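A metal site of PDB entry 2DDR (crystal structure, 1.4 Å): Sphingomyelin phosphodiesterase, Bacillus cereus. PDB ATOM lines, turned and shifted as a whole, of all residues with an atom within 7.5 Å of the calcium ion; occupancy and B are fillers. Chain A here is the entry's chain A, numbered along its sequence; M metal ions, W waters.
The side-chain amide oxygen (OD1) of Asn 57 sits close to the guanidinium group (NE) of Arg 80, 3.4 Å away. The backbone carbonyl oxygen of Asn 57 lies within hydrogen-bond range of the side-chain hydroxyl of Ser 60 (3.0 Å). The backbone carbonyl oxygen of Met 19 lies within hydrogen-bond range of the backbone NH of Phe 55. The side-chain carboxylate (OD2) of Asp 100 sits close to the guanidinium group (NE) of Arg 80 (2.8 Å). OD1 of Asp 100 lies within hydrogen-bond range of N of Gly 102, 2.8 Å away. The backbone carbonyl oxygen (O) of Val 54 is in hydrogen-bond range of the guanidinium group (NH2) of Arg 80 (3.0 Å). The guanidinium group of Arg 80 is in hydrogen-bond range of the side-chain hydroxyl of Ser 60 (3.0 Å).
Arg 80 touches the calcium ion (NH2 to CA, 3.8 Å). Of the 17 residues printed, 5 come within 4 Å of the calcium ion. The nearest printed residue that does not touch the calcium ion is Asp 56 (4.5 Å).
The calcium ion is bound by the side-chain amide oxygen (OD1) of Asn 57 (2.3 Å), the backbone carbonyl oxygen (O) of Phe 55 (2.3 Å), the side-chain carboxylate (OE1) of Glu 99 (2.3 Å), the side-chain carboxylate (OD2) of Asp 100 (2.3 Å), water W1 (2.3 Å) and water W2 (2.4 Å).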
ATOM      1  N   MET A  19      19.008   7.752   2.887  1.00  0.00           N
ATOM      2  CA  MET A  19      18.429   6.699   3.718  1.00  0.00           C
ATOM      3  C   MET A  19      17.105   7.170   4.269  1.00  0.00           C
ATOM      4  O   MET A  19      16.978   7.501   5.448  1.00  0.00           O
ATOM      5  CB  MET A  19      19.379   6.328   4.858  1.00  0.00           C
ATOM      6  CG  MET A  19      20.708   5.799   4.377  1.00  0.00           C
ATOM      7  SD  MET A  19      21.540   4.880   5.657  1.00  0.00           S
ATOM      8  CE  MET A  19      22.339   3.617   4.686  1.00  0.00           C
ATOM      9  N   SER A  21      13.216   7.124   5.568  1.00  0.00           N
ATOM     10  CA  SER A  21      12.602   6.273   6.568  1.00  0.00           C
ATOM     11  C   SER A  21      11.944   5.054   5.930  1.00  0.00           C
ATOM     12  O   SER A  21      11.237   5.190   4.918  1.00  0.00           O
ATOM     13  CB  SER A  21      11.541   7.041   7.354  1.00  0.00           C
ATOM     14  OG  SER A  21      10.866   6.169   8.246  1.00  0.00           O
ATOM     15  N   VAL A  54      20.512  10.531   6.755  1.00  0.00           N
ATOM     16  CA  VAL A  54      20.526   9.287   7.518  1.00  0.00           C
ATOM     17  C   VAL A  54      19.260   9.369   8.374  1.00  0.00           C
ATOM     18  O   VAL A  54      19.321   9.392   9.607  1.00  0.00           O
ATOM     19  CB  VAL A  54      21.801   9.148   8.409  1.00  0.00           C
ATOM     20  CG1 VAL A  54      22.968   8.664   7.560  1.00  0.00           C
ATOM     21  CG2 VAL A  54      22.144  10.481   9.056  1.00  0.00           C
ATOM     22  N   PHE A  55      18.120   9.411   7.696  1.00  0.00           N
ATOM     23  CA  PHE A  55      16.823   9.541   8.344  1.00  0.00           C
ATOM     24  C   PHE A  55      16.276   8.277   9.004  1.00  0.00           C
ATOM     25  O   PHE A  55      15.742   8.352  10.123  1.00  0.00           O
ATOM     26  CB  PHE A  55      15.757  10.023   7.344  1.00  0.00           C
ATOM     27  CG  PHE A  55      16.034  11.362   6.737  1.00  0.00           C
ATOM     28  CD1 PHE A  55      16.176  11.500   5.369  1.00  0.00           C
ATOM     29  CD2 PHE A  55      16.114  12.504   7.541  1.00  0.00           C
ATOM     30  CE1 PHE A  55      16.377  12.747   4.791  1.00  0.00           C
ATOM     31  CE2 PHE A  55      16.319  13.761   6.964  1.00  0.00           C
ATOM     32  CZ  PHE A  55      16.448  13.884   5.585  1.00  0.00           C
ATOM     33  N   ASP A  56      16.373   7.141   8.334  1.00  0.00           N
ATOM     34  CA  ASP A  56      15.850   5.911   8.921  1.00  0.00           C
ATOM     35  C   ASP A  56      16.613   5.618  10.191  1.00  0.00           C
ATOM     36  O   ASP A  56      17.839   5.524  10.167  1.00  0.00           O
ATOM     37  CB  ASP A  56      15.979   4.727   7.965  1.00  0.00           C
ATOM     38  CG  ASP A  56      15.308   3.486   8.497  1.00  0.00           C
ATOM     39  OD1 ASP A  56      14.065   3.493   8.629  1.00  0.00           O
ATOM     40  OD2 ASP A  56      16.005   2.503   8.817  1.00  0.00           O
ATOM     41  N   ASN A  57      15.902   5.466  11.302  1.00  0.00           N
ATOM     42  CA  ASN A  57      16.579   5.225  12.570  1.00  0.00           C
ATOM     43  C   ASN A  57      17.394   3.940  12.616  1.00  0.00           C
ATOM     44  O   ASN A  57      18.554   3.955  13.011  1.00  0.00           O
ATOM     45  CB  ASN A  57      15.552   5.251  13.707  1.00  0.00           C
ATOM     46  CG  ASN A  57      15.037   6.655  13.995  1.00  0.00           C
ATOM     47  OD1 ASN A  57      15.199   7.556  13.180  1.00  0.00           O
ATOM     48  ND2 ASN A  57      14.404   6.829  15.141  1.00  0.00           N
ATOM     49  N   SER A  58      16.796   2.821  12.221  1.00  0.00           N
ATOM     50  CA  SER A  58      17.499   1.546  12.251  1.00  0.00           C
ATOM     51  C   SER A  58      18.684   1.473  11.298  1.00  0.00           C
ATOM     52  O   SER A  58      19.781   1.073  11.686  1.00  0.00           O
ATOM     53  CB  SER A  58      16.532   0.398  11.946  1.00  0.00           C
ATOM     54  OG  SER A  58      15.591   0.241  12.991  1.00  0.00           O
ATOM     55  N   SER A  60      20.299   3.982   9.889  1.00  0.00           N
ATOM     56  CA  SER A  60      21.337   4.960  10.214  1.00  0.00           C
ATOM     57  C   SER A  60      22.213   4.457  11.353  1.00  0.00           C
ATOM     58  O   SER A  60      23.430   4.593  11.310  1.00  0.00           O
ATOM     59  CB  SER A  60      20.728   6.323  10.551  1.00  0.00           C
ATOM     60  OG  SER A  60      19.971   6.301  11.746  1.00  0.00           O
ATOM     61  N   VAL A  77      22.508  11.804  15.647  1.00  0.00           N
ATOM     62  CA  VAL A  77      21.929  12.317  14.415  1.00  0.00           C
ATOM     63  C   VAL A  77      21.133  13.583  14.720  1.00  0.00           C
ATOM     64  O   VAL A  77      20.260  13.602  15.580  1.00  0.00           O
ATOM     65  CB  VAL A  77      21.016  11.279  13.744  1.00  0.00           C
ATOM     66  CG1 VAL A  77      20.318  11.879  12.520  1.00  0.00           C
ATOM     67  CG2 VAL A  77      21.836  10.077  13.318  1.00  0.00           C
ATOM     68  N   LEU A  78      21.470  14.652  14.011  1.00  0.00           N
ATOM     69  CA  LEU A  78      20.814  15.944  14.159  1.00  0.00           C
ATOM     70  C   LEU A  78      19.298  15.831  14.311  1.00  0.00           C
ATOM     71  O   LEU A  78      18.646  15.157  13.522  1.00  0.00           O
ATOM     72  CB  LEU A  78      21.107  16.804  12.929  1.00  0.00           C
ATOM     73  CG  LEU A  78      20.241  18.046  12.745  1.00  0.00           C
ATOM     74  CD1 LEU A  78      20.616  19.092  13.769  1.00  0.00           C
ATOM     75  CD2 LEU A  78      20.407  18.602  11.347  1.00  0.00           C
ATOM     76  N   GLY A  79      18.759  16.482  15.336  1.00  0.00           N
ATOM     77  CA  GLY A  79      17.322  16.501  15.549  1.00  0.00           C
ATOM     78  C   GLY A  79      16.591  15.255  16.002  1.00  0.00           C
ATOM     79  O   GLY A  79      15.358  15.225  15.989  1.00  0.00           O
ATOM     80  N   ARG A  80      17.316  14.222  16.419  1.00  0.00           N
ATOM     81  CA  ARG A  80      16.663  12.997  16.862  1.00  0.00           C
ATOM     82  C   ARG A  80      16.458  12.967  18.374  1.00  0.00           C
ATOM     83  O   ARG A  80      15.614  12.235  18.881  1.00  0.00           O
ATOM     84  CB  ARG A  80      17.494  11.781  16.422  1.00  0.00           C
ATOM     85  CG  ARG A  80      16.760  10.452  16.559  1.00  0.00           C
ATOM     86  CD  ARG A  80      17.571   9.306  15.952  1.00  0.00           C
ATOM     87  NE  ARG A  80      17.682   9.415  14.503  1.00  0.00           N
ATOM     88  CZ  ARG A  80      18.413   8.596  13.751  1.00  0.00           C
ATOM     89  NH1 ARG A  80      19.108   7.601  14.301  1.00  0.00           N
ATOM     90  NH2 ARG A  80      18.449   8.765  12.433  1.00  0.00           N
ATOM     91  N   PRO A  98       8.014  14.766  12.832  1.00  0.00           N
ATOM     92  CA  PRO A  98       7.874  13.372  12.385  1.00  0.00           C
ATOM     93  C   PRO A  98       9.204  12.742  11.971  1.00  0.00           C
ATOM     94  O   PRO A  98       9.309  11.524  11.879  1.00  0.00           O
ATOM     95  CB  PRO A  98       6.912  13.477  11.199  1.00  0.00           C
ATOM     96  CG  PRO A  98       6.149  14.745  11.461  1.00  0.00           C
ATOM     97  CD  PRO A  98       7.229  15.665  11.959  1.00  0.00           C
ATOM     98  N   GLU A  99      10.202  13.574  11.715  1.00  0.00           N
ATOM     99  CA  GLU A  99      11.509  13.107  11.261  1.00  0.00           C
ATOM    100  C   GLU A  99      12.639  13.959  11.825  1.00  0.00           C
ATOM    101  O   GLU A  99      12.412  15.094  12.248  1.00  0.00           O
ATOM    102  CB  GLU A  99      11.553  13.128   9.727  1.00  0.00           C
ATOM    103  CG  GLU A  99      12.810  12.556   9.097  1.00  0.00           C
ATOM    104  CD  GLU A  99      13.100  11.160   9.572  1.00  0.00           C
ATOM    105  OE1 GLU A  99      13.935  11.001  10.488  1.00  0.00           O
ATOM    106  OE2 GLU A  99      12.481  10.205   9.051  1.00  0.00           O
ATOM    107  N   ASP A 100      13.854  13.420  11.825  1.00  0.00           N
ATOM    108  CA  ASP A 100      15.011  14.158  12.324  1.00  0.00           C
ATOM    109  C   ASP A 100      15.720  14.878  11.163  1.00  0.00           C
ATOM    110  O   ASP A 100      15.265  14.813  10.029  1.00  0.00           O
ATOM    111  CB  ASP A 100      15.985  13.226  13.048  1.00  0.00           C
ATOM    112  CG  ASP A 100      16.464  12.066  12.171  1.00  0.00           C
ATOM    113  OD1 ASP A 100      17.064  12.320  11.106  1.00  0.00           O
ATOM    114  OD2 ASP A 100      16.250  10.899  12.568  1.00  0.00           O
ATOM    115  N   GLY A 101      16.817  15.564  11.464  1.00  0.00           N
ATOM    116  CA  GLY A 101      17.553  16.302  10.455  1.00  0.00           C
ATOM    117  C   GLY A 101      18.404  15.470   9.504  1.00  0.00           C
ATOM    118  O   GLY A 101      18.847  15.983   8.469  1.00  0.00           O
ATOM    119  N   GLY A 102      18.670  14.225   9.873  1.00  0.00           N
ATOM    120  CA  GLY A 102      19.451  13.342   9.027  1.00  0.00           C
ATOM    121  C   GLY A 102      20.931  13.636   8.826  1.00  0.00           C
ATOM    122  O   GLY A 102      21.548  13.100   7.904  1.00  0.00           O
HETATM  123 CA    CA M   1      14.707   9.335  11.875  1.00  0.00          CA
HETATM  124  O   HOH W   1      13.291  10.265  13.468  1.00  0.00           O
HETATM  125  O   HOH W   2      12.719   8.350  10.962  1.00  0.00           O
